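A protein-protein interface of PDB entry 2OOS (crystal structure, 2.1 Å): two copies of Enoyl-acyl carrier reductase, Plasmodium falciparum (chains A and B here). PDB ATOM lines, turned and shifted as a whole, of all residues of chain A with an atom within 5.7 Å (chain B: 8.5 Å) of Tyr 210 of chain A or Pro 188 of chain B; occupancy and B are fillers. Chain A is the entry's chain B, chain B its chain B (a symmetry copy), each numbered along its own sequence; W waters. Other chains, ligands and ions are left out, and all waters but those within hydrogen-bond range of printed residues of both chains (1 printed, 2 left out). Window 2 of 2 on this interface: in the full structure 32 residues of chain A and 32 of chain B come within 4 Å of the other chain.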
ATOM      1  N   THR A 205      33.537  -8.332  35.186  1.00  0.00           N
ATOM      2  CA  THR A 205      34.790  -8.759  34.545  1.00  0.00           C
ATOM      3  C   THR A 205      34.524  -9.321  33.134  1.00  0.00           C
ATOM      4  O   THR A 205      35.269  -9.041  32.190  1.00  0.00           O
ATOM      5  CB  THR A 205      35.544  -9.782  35.461  1.00  0.00           C
ATOM      6  OG1 THR A 205      36.004  -9.113  36.649  1.00  0.00           O
ATOM      7  CG2 THR A 205      36.745 -10.411  34.719  1.00  0.00           C
ATOM      8  N   ARG A 206      33.455 -10.090  32.992  1.00  0.00           N
ATOM      9  CA  ARG A 206      32.982 -10.549  31.659  1.00  0.00           C
ATOM     10  C   ARG A 206      32.520  -9.410  30.739  1.00  0.00           C
ATOM     11  O   ARG A 206      33.023  -9.281  29.601  1.00  0.00           O
ATOM     12  CB  ARG A 206      31.842 -11.555  31.773  1.00  0.00           C
ATOM     13  CG  ARG A 206      32.265 -12.933  32.289  1.00  0.00           C
ATOM     14  CD  ARG A 206      31.074 -13.851  32.307  1.00  0.00           C
ATOM     15  NE  ARG A 206      30.147 -13.552  33.445  1.00  0.00           N
ATOM     16  CZ  ARG A 206      30.265 -14.135  34.632  1.00  0.00           C
ATOM     17  NH1 ARG A 206      31.263 -14.998  34.818  1.00  0.00           N
ATOM     18  NH2 ARG A 206      29.405 -13.873  35.613  1.00  0.00           N
ATOM     19  N   VAL A 207      31.588  -8.590  31.215  1.00  0.00           N
ATOM     20  CA  VAL A 207      31.064  -7.448  30.390  1.00  0.00           C
ATOM     21  C   VAL A 207      32.182  -6.466  29.952  1.00  0.00           C
ATOM     22  O   VAL A 207      32.266  -6.087  28.763  1.00  0.00           O
ATOM     23  CB  VAL A 207      29.929  -6.722  31.147  1.00  0.00           C
ATOM     24  CG1 VAL A 207      29.359  -5.529  30.314  1.00  0.00           C
ATOM     25  CG2 VAL A 207      28.815  -7.755  31.470  1.00  0.00           C
ATOM     26  N   LEU A 208      33.027  -6.077  30.901  1.00  0.00           N
ATOM     27  CA  LEU A 208      34.236  -5.282  30.641  1.00  0.00           C
ATOM     28  C   LEU A 208      35.142  -5.945  29.613  1.00  0.00           C
ATOM     29  O   LEU A 208      35.652  -5.285  28.713  1.00  0.00           O
ATOM     30  CB  LEU A 208      35.028  -4.970  31.925  1.00  0.00           C
ATOM     31  CG  LEU A 208      34.266  -4.024  32.886  1.00  0.00           C
ATOM     32  CD1 LEU A 208      34.921  -3.923  34.246  1.00  0.00           C
ATOM     33  CD2 LEU A 208      34.047  -2.646  32.304  1.00  0.00           C
ATOM     34  N   ALA A 209      35.326  -7.265  29.736  1.00  0.00           N
ATOM     35  CA  ALA A 209      36.187  -7.981  28.812  1.00  0.00           C
ATOM     36  C   ALA A 209      35.654  -7.849  27.376  1.00  0.00           C
ATOM     37  O   ALA A 209      36.453  -7.684  26.448  1.00  0.00           O
ATOM     38  CB  ALA A 209      36.370  -9.457  29.218  1.00  0.00           C
ATOM     39  N   TYR A 210      34.337  -7.927  27.209  1.00  0.00           N
ATOM     40  CA  TYR A 210      33.707  -7.697  25.928  1.00  0.00           C
ATOM     41  C   TYR A 210      34.017  -6.286  25.370  1.00  0.00           C
ATOM     42  O   TYR A 210      34.524  -6.172  24.241  1.00  0.00           O
ATOM     43  CB  TYR A 210      32.199  -7.945  25.985  1.00  0.00           C
ATOM     44  CG  TYR A 210      31.501  -7.524  24.705  1.00  0.00           C
ATOM     45  CD1 TYR A 210      31.576  -8.298  23.556  1.00  0.00           C
ATOM     46  CD2 TYR A 210      30.765  -6.341  24.650  1.00  0.00           C
ATOM     47  CE1 TYR A 210      30.921  -7.919  22.387  1.00  0.00           C
ATOM     48  CE2 TYR A 210      30.143  -5.922  23.458  1.00  0.00           C
ATOM     49  CZ  TYR A 210      30.228  -6.716  22.348  1.00  0.00           C
ATOM     50  OH  TYR A 210      29.597  -6.333  21.202  1.00  0.00           O
ATOM     51  N   HIS A 211      33.697  -5.234  26.141  1.00  0.00           N
ATOM     52  CA  HIS A 211      33.909  -3.855  25.702  1.00  0.00           C
ATOM     53  C   HIS A 211      35.386  -3.478  25.481  1.00  0.00           C
ATOM     54  O   HIS A 211      35.731  -2.830  24.478  1.00  0.00           O
ATOM     55  CB  HIS A 211      33.239  -2.831  26.656  1.00  0.00           C
ATOM     56  CG  HIS A 211      31.753  -2.966  26.735  1.00  0.00           C
ATOM     57  ND1 HIS A 211      30.925  -2.839  25.634  1.00  0.00           N
ATOM     58  CD2 HIS A 211      30.939  -3.192  27.793  1.00  0.00           C
ATOM     59  CE1 HIS A 211      29.673  -3.039  26.004  1.00  0.00           C
ATOM     60  NE2 HIS A 211      29.655  -3.242  27.310  1.00  0.00           N
ATOM     61  N   LEU A 212      36.237  -3.849  26.433  1.00  0.00           N
ATOM     62  CA  LEU A 212      37.670  -3.566  26.382  1.00  0.00           C
ATOM     63  C   LEU A 212      38.394  -4.337  25.286  1.00  0.00           C
ATOM     64  O   LEU A 212      39.335  -3.817  24.668  1.00  0.00           O
ATOM     65  CB  LEU A 212      38.347  -3.805  27.752  1.00  0.00           C
ATOM     66  CG  LEU A 212      37.808  -2.921  28.904  1.00  0.00           C
ATOM     67  CD1 LEU A 212      38.438  -3.355  30.223  1.00  0.00           C
ATOM     68  CD2 LEU A 212      38.094  -1.434  28.668  1.00  0.00           C
ATOM     69  N   GLY A 213      37.981  -5.574  25.061  1.00  0.00           N
ATOM     70  CA  GLY A 213      38.596  -6.389  24.029  1.00  0.00           C
ATOM     71  C   GLY A 213      38.287  -5.835  22.650  1.00  0.00           C
ATOM     72  O   GLY A 213      39.193  -5.647  21.844  1.00  0.00           O
ATOM     73  N   ARG A 214      37.008  -5.572  22.401  1.00  0.00           N
ATOM     74  CA  ARG A 214      36.540  -5.084  21.100  1.00  0.00           C
ATOM     75  C   ARG A 214      37.024  -3.710  20.729  1.00  0.00           C
ATOM     76  O   ARG A 214      37.358  -3.493  19.584  1.00  0.00           O
ATOM     77  CB  ARG A 214      35.023  -5.025  21.052  1.00  0.00           C
ATOM     78  CG  ARG A 214      34.399  -6.354  21.172  1.00  0.00           C
ATOM     79  CD  ARG A 214      34.720  -7.208  19.985  1.00  0.00           C
ATOM     80  NE  ARG A 214      33.555  -8.039  19.851  1.00  0.00           N
ATOM     81  CZ  ARG A 214      33.290  -8.866  18.855  1.00  0.00           C
ATOM     82  NH1 ARG A 214      34.137  -9.006  17.837  1.00  0.00           N
ATOM     83  NH2 ARG A 214      32.158  -9.568  18.911  1.00  0.00           N
ATOM     84  N   ASN A 215      37.046  -2.799  21.702  1.00  0.00           N
ATOM     85  CA  ASN A 215      37.276  -1.409  21.432  1.00  0.00           C
ATOM     86  C   ASN A 215      38.702  -0.996  21.639  1.00  0.00           C
ATOM     87  O   ASN A 215      39.148  -0.005  21.028  1.00  0.00           O
ATOM     88  CB  ASN A 215      36.310  -0.515  22.239  1.00  0.00           C
ATOM     89  CG  ASN A 215      34.837  -0.738  21.845  1.00  0.00           C
ATOM     90  OD1 ASN A 215      33.979  -0.889  22.700  1.00  0.00           O
ATOM     91  ND2 ASN A 215      34.557  -0.760  20.561  1.00  0.00           N
ATOM     92  N   VAL B 135      20.313   2.309  32.148  1.00  0.00           N
ATOM     93  CA  VAL B 135      20.227   0.991  31.488  1.00  0.00           C
ATOM     94  C   VAL B 135      20.703   1.054  30.036  1.00  0.00           C
ATOM     95  O   VAL B 135      21.209   0.062  29.511  1.00  0.00           O
ATOM     96  CB  VAL B 135      18.772   0.354  31.621  1.00  0.00           C
ATOM     97  CG1 VAL B 135      17.666   1.273  31.049  1.00  0.00           C
ATOM     98  CG2 VAL B 135      18.670  -0.997  31.029  1.00  0.00           C
ATOM     99  N   LYS B 137      23.139   2.881  28.839  1.00  0.00           N
ATOM    100  CA  LYS B 137      24.575   3.018  28.734  1.00  0.00           C
ATOM    101  C   LYS B 137      25.210   1.660  28.915  1.00  0.00           C
ATOM    102  O   LYS B 137      24.769   0.849  29.781  1.00  0.00           O
ATOM    103  CB  LYS B 137      25.089   3.959  29.819  1.00  0.00           C
ATOM    104  CG  LYS B 137      24.400   5.319  29.756  1.00  0.00           C
ATOM    105  CD  LYS B 137      25.226   6.418  30.399  1.00  0.00           C
ATOM    106  CE  LYS B 137      24.488   7.781  30.408  1.00  0.00           C
ATOM    107  NZ  LYS B 137      25.415   8.827  31.001  1.00  0.00           N
ATOM    108  N   ASP B 138      26.278   1.403  28.172  1.00  0.00           N
ATOM    109  CA  ASP B 138      26.982   0.180  28.473  1.00  0.00           C
ATOM    110  C   ASP B 138      27.696   0.328  29.800  1.00  0.00           C
ATOM    111  O   ASP B 138      27.877   1.442  30.305  1.00  0.00           O
ATOM    112  CB  ASP B 138      27.880  -0.303  27.312  1.00  0.00           C
ATOM    113  CG  ASP B 138      28.902   0.685  26.920  1.00  0.00           C
ATOM    114  OD1 ASP B 138      29.056   0.895  25.675  1.00  0.00           O
ATOM    115  OD2 ASP B 138      29.586   1.198  27.821  1.00  0.00           O
ATOM    116  N   LEU B 139      28.078  -0.799  30.371  1.00  0.00           N
ATOM    117  CA  LEU B 139      28.650  -0.842  31.726  1.00  0.00           C
ATOM    118  C   LEU B 139      29.829   0.094  31.918  1.00  0.00           C
ATOM    119  O   LEU B 139      29.895   0.851  32.890  1.00  0.00           O
ATOM    120  CB  LEU B 139      29.131  -2.273  32.009  1.00  0.00           C
ATOM    121  CG  LEU B 139      28.906  -2.919  33.365  1.00  0.00           C
ATOM    122  CD1 LEU B 139      30.125  -3.784  33.779  1.00  0.00           C
ATOM    123  CD2 LEU B 139      28.402  -1.939  34.455  1.00  0.00           C
ATOM    124  N   LEU B 140      30.776   0.027  30.975  1.00  0.00           N
ATOM    125  CA  LEU B 140      31.972   0.871  30.993  1.00  0.00           C
ATOM    126  C   LEU B 140      31.672   2.358  31.092  1.00  0.00           C
ATOM    127  O   LEU B 140      32.435   3.103  31.700  1.00  0.00           O
ATOM    128  CB  LEU B 140      32.744   0.657  29.702  1.00  0.00           C
ATOM    129  CG  LEU B 140      34.261   0.551  29.623  1.00  0.00           C
ATOM    130  CD1 LEU B 140      34.732   1.027  28.250  1.00  0.00           C
ATOM    131  CD2 LEU B 140      35.079   1.105  30.860  1.00  0.00           C
ATOM    132  N   TYR B 180      17.957 -12.567  34.946  1.00  0.00           N
ATOM    133  CA  TYR B 180      18.235 -12.718  33.510  1.00  0.00           C
ATOM    134  C   TYR B 180      19.682 -13.202  33.295  1.00  0.00           C
ATOM    135  O   TYR B 180      20.582 -12.781  34.033  1.00  0.00           O
ATOM    136  CB  TYR B 180      17.880 -11.412  32.743  1.00  0.00           C
ATOM    137  CG  TYR B 180      18.081 -11.514  31.242  1.00  0.00           C
ATOM    138  CD1 TYR B 180      17.403 -12.457  30.484  1.00  0.00           C
ATOM    139  CD2 TYR B 180      19.013 -10.700  30.607  1.00  0.00           C
ATOM    140  CE1 TYR B 180      17.632 -12.577  29.116  1.00  0.00           C
ATOM    141  CE2 TYR B 180      19.251 -10.790  29.258  1.00  0.00           C
ATOM    142  CZ  TYR B 180      18.547 -11.732  28.518  1.00  0.00           C
ATOM    143  OH  TYR B 180      18.787 -11.835  27.169  1.00  0.00           O
ATOM    144  N   ALA B 182      22.087 -12.544  31.420  1.00  0.00           N
ATOM    145  CA  ALA B 182      23.154 -11.527  31.291  1.00  0.00           C
ATOM    146  C   ALA B 182      24.022 -11.364  32.537  1.00  0.00           C
ATOM    147  O   ALA B 182      25.110 -10.799  32.438  1.00  0.00           O
ATOM    148  CB  ALA B 182      22.574 -10.201  30.915  1.00  0.00           C
ATOM    149  N   LYS B 185      26.416 -14.509  31.320  1.00  0.00           N
ATOM    150  CA  LYS B 185      27.023 -14.481  29.962  1.00  0.00           C
ATOM    151  C   LYS B 185      26.712 -13.111  29.354  1.00  0.00           C
ATOM    152  O   LYS B 185      25.697 -12.557  29.684  1.00  0.00           O
ATOM    153  CB  LYS B 185      26.454 -15.581  29.060  1.00  0.00           C
ATOM    154  CG  LYS B 185      26.803 -17.035  29.409  1.00  0.00           C
ATOM    155  CD  LYS B 185      28.326 -17.309  29.477  1.00  0.00           C
ATOM    156  CE  LYS B 185      28.592 -18.807  29.927  1.00  0.00           C
ATOM    157  NZ  LYS B 185      30.051 -19.064  30.086  1.00  0.00           N
ATOM    158  N   VAL B 186      27.599 -12.566  28.501  1.00  0.00           N
ATOM    159  CA  VAL B 186      27.477 -11.162  28.077  1.00  0.00           C
ATOM    160  C   VAL B 186      26.345 -10.969  27.076  1.00  0.00           C
ATOM    161  O   VAL B 186      26.243 -11.729  26.106  1.00  0.00           O
ATOM    162  CB  VAL B 186      28.830 -10.575  27.566  1.00  0.00           C
ATOM    163  CG1 VAL B 186      28.701  -9.050  27.221  1.00  0.00           C
ATOM    164  CG2 VAL B 186      29.952 -10.803  28.618  1.00  0.00           C
ATOM    165  N   VAL B 187      25.470 -10.009  27.413  1.00  0.00           N
ATOM    166  CA  VAL B 187      24.413  -9.460  26.553  1.00  0.00           C
ATOM    167  C   VAL B 187      24.723  -7.978  26.396  1.00  0.00           C
ATOM    168  O   VAL B 187      24.433  -7.181  27.297  1.00  0.00           O
ATOM    169  CB  VAL B 187      22.970  -9.683  27.155  1.00  0.00           C
ATOM    170  CG1 VAL B 187      21.870  -9.001  26.279  1.00  0.00           C
ATOM    171  CG2 VAL B 187      22.645 -11.189  27.239  1.00  0.00           C
ATOM    172  N   PRO B 188      25.404  -7.596  25.285  1.00  0.00           N
ATOM    173  CA  PRO B 188      25.614  -6.162  25.024  1.00  0.00           C
ATOM    174  C   PRO B 188      24.211  -5.527  24.882  1.00  0.00           C
ATOM    175  O   PRO B 188      23.310  -6.124  24.290  1.00  0.00           O
ATOM    176  CB  PRO B 188      26.376  -6.147  23.683  1.00  0.00           C
ATOM    177  CG  PRO B 188      26.950  -7.550  23.568  1.00  0.00           C
ATOM    178  CD  PRO B 188      25.992  -8.444  24.236  1.00  0.00           C
ATOM    179  N   GLY B 189      24.023  -4.369  25.476  1.00  0.00           N
ATOM    180  CA  GLY B 189      22.704  -3.704  25.478  1.00  0.00           C
ATOM    181  C   GLY B 189      21.975  -3.801  26.823  1.00  0.00           C
ATOM    182  O   GLY B 189      21.040  -3.029  27.074  1.00  0.00           O
ATOM    183  N   TYR B 190      22.342  -4.799  27.651  1.00  0.00           N
ATOM    184  CA  TYR B 190      21.774  -4.948  29.002  1.00  0.00           C
ATOM    185  C   TYR B 190      22.636  -4.108  29.915  1.00  0.00           C
ATOM    186  O   TYR B 190      23.551  -4.619  30.612  1.00  0.00           O
ATOM    187  CB  TYR B 190      21.789  -6.414  29.433  1.00  0.00           C
ATOM    188  CG  TYR B 190      20.818  -6.759  30.575  1.00  0.00           C
ATOM    189  CD1 TYR B 190      19.415  -6.651  30.401  1.00  0.00           C
ATOM    190  CD2 TYR B 190      21.297  -7.191  31.821  1.00  0.00           C
ATOM    191  CE1 TYR B 190      18.529  -7.021  31.439  1.00  0.00           C
ATOM    192  CE2 TYR B 190      20.395  -7.571  32.881  1.00  0.00           C
ATOM    193  CZ  TYR B 190      19.044  -7.450  32.682  1.00  0.00           C
ATOM    194  OH  TYR B 190      18.186  -7.792  33.677  1.00  0.00           O
ATOM    195  N   GLY B 191      22.380  -2.806  29.887  1.00  0.00           N
ATOM    196  CA  GLY B 191      23.358  -1.859  30.363  1.00  0.00           C
ATOM    197  C   GLY B 191      23.103  -1.324  31.754  1.00  0.00           C
ATOM    198  O   GLY B 191      22.238  -1.808  32.470  1.00  0.00           O
ATOM    199  N   SER B 195      23.288  -5.948  34.472  1.00  0.00           N
ATOM    200  CA  SER B 195      23.929  -7.251  34.443  1.00  0.00           C
ATOM    201  C   SER B 195      24.520  -7.519  35.845  1.00  0.00           C
ATOM    202  O   SER B 195      24.387  -8.637  36.392  1.00  0.00           O
ATOM    203  CB  SER B 195      25.032  -7.274  33.372  1.00  0.00           C
ATOM    204  OG  SER B 195      26.042  -6.273  33.644  1.00  0.00           O
ATOM    205  N   ILE B 236      13.636  -0.074  26.565  1.00  0.00           N
ATOM    206  CA  ILE B 236      15.091  -0.154  26.444  1.00  0.00           C
ATOM    207  C   ILE B 236      15.524  -0.106  24.963  1.00  0.00           C
ATOM    208  O   ILE B 236      15.259  -1.039  24.207  1.00  0.00           O
ATOM    209  CB  ILE B 236      15.652  -1.427  27.181  1.00  0.00           C
ATOM    210  CG1 ILE B 236      15.224  -1.434  28.648  1.00  0.00           C
ATOM    211  CG2 ILE B 236      17.176  -1.531  27.063  1.00  0.00           C
ATOM    212  CD1 ILE B 236      15.377  -2.822  29.331  1.00  0.00           C
ATOM    213  N   ASN B 237      16.187   1.003  24.605  1.00  0.00           N
ATOM    214  CA  ASN B 237      16.735   1.377  23.266  1.00  0.00           C
ATOM    215  C   ASN B 237      17.691   0.302  22.737  1.00  0.00           C
ATOM    216  O   ASN B 237      18.812   0.132  23.256  1.00  0.00           O
ATOM    217  CB  ASN B 237      17.525   2.709  23.458  1.00  0.00           C
ATOM    218  CG  ASN B 237      17.934   3.412  22.140  1.00  0.00           C
ATOM    219  OD1 ASN B 237      19.115   3.378  21.749  1.00  0.00           O
ATOM    220  ND2 ASN B 237      16.989   4.118  21.508  1.00  0.00           N
ATOM    221  N   PHE B 281      15.826  -3.953  21.141  1.00  0.00           N
ATOM    222  CA  PHE B 281      16.571  -5.188  21.355  1.00  0.00           C
ATOM    223  C   PHE B 281      15.579  -6.295  21.787  1.00  0.00           C
ATOM    224  O   PHE B 281      15.810  -7.445  21.496  1.00  0.00           O
ATOM    225  CB  PHE B 281      17.709  -5.045  22.392  1.00  0.00           C
ATOM    226  CG  PHE B 281      18.593  -6.298  22.508  1.00  0.00           C
ATOM    227  CD1 PHE B 281      19.633  -6.538  21.604  1.00  0.00           C
ATOM    228  CD2 PHE B 281      18.365  -7.257  23.502  1.00  0.00           C
ATOM    229  CE1 PHE B 281      20.438  -7.715  21.709  1.00  0.00           C
ATOM    230  CE2 PHE B 281      19.169  -8.424  23.616  1.00  0.00           C
ATOM    231  CZ  PHE B 281      20.200  -8.653  22.713  1.00  0.00           C
ATOM    232  N   TYR B 284      14.302  -8.333  18.789  1.00  0.00           N
ATOM    233  CA  TYR B 284      15.442  -9.163  18.423  1.00  0.00           C
ATOM    234  C   TYR B 284      15.651 -10.331  19.396  1.00  0.00           C
ATOM    235  O   TYR B 284      15.780 -11.491  18.967  1.00  0.00           O
ATOM    236  CB  TYR B 284      16.745  -8.340  18.309  1.00  0.00           C
ATOM    237  CG  TYR B 284      18.003  -9.206  18.114  1.00  0.00           C
ATOM    238  CD1 TYR B 284      18.159 -10.031  16.979  1.00  0.00           C
ATOM    239  CD2 TYR B 284      19.030  -9.211  19.065  1.00  0.00           C
ATOM    240  CE1 TYR B 284      19.318 -10.828  16.798  1.00  0.00           C
ATOM    241  CE2 TYR B 284      20.185 -10.005  18.899  1.00  0.00           C
ATOM    242  CZ  TYR B 284      20.322 -10.807  17.771  1.00  0.00           C
ATOM    243  OH  TYR B 284      21.470 -11.590  17.606  1.00  0.00           O
HETATM  244  O   HOH W   1      27.086  -3.493  28.794  1.00  0.00           O
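Among the printed residues, merely in contact across the chains: Arg 206 of chain A with Val 186 of chain B, Val 207 of chain A with Leu 139 of chain B, Val 207 of chain A with Val 186 of chain B, Val 207 of chain A with Ser 195 of chain B, Tyr 210 of chain A with Val 186 of chain B, Tyr 210 of chain A with Pro 188 of chain B and His 211 of chain A with Asp 138 of chain B.
Tyr 210 of chain A touches two residues of chain B.
Pro 188 of chain B touches one residue of chain A.
Printed residues of chain B within 4 Å of Arg 206 of chain A: Val 186.
Printed residues of chain A within 4 Å of Leu 139 of chain B: Val 207 (3.7 Å).
Of the printed residues of chain A, Asp 138 of chain B touches His 211 (3.4 Å).
The nearest residue of chain A that does not touch Pro 188 of chain B is His 211 of chain A (5.1 Å).
No position is printed for both chains.
Of the 7 pairs that touch across the chains among the printed residues, none has its exchanged pair printed and touching as well.
Of the 11 printed residues of chain A, 4 touch a printed residue of chain B.
Printed residues of chain A that touch a printed residue of chain B: Arg 206, Val 207, Tyr 210 and His 211.
Hydrophobic or aromatic side chains of chain A that line the printed part of chain B: Val 207, Tyr 210 and His 211.
Hydrophobic or aromatic side chains of chain B within 4 Å of the printed part of chain A: Leu 139, Val 186 and Pro 188.
Among the printed residues, 7 pairs touch across the chains.
Among the printed residues, no Asp or Glu carboxylate lies within 4 Å of a Lys or Arg side-chain nitrogen of the other chain.
Water W1 bridges a ring nitrogen (NE2) of His 211 of chain A (3.0 Å) and the backbone NH (N) of Leu 139 of chain B (3.3 Å).
O of His 211 of chain A lies close to OD1 of Asn 215 of chain A.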
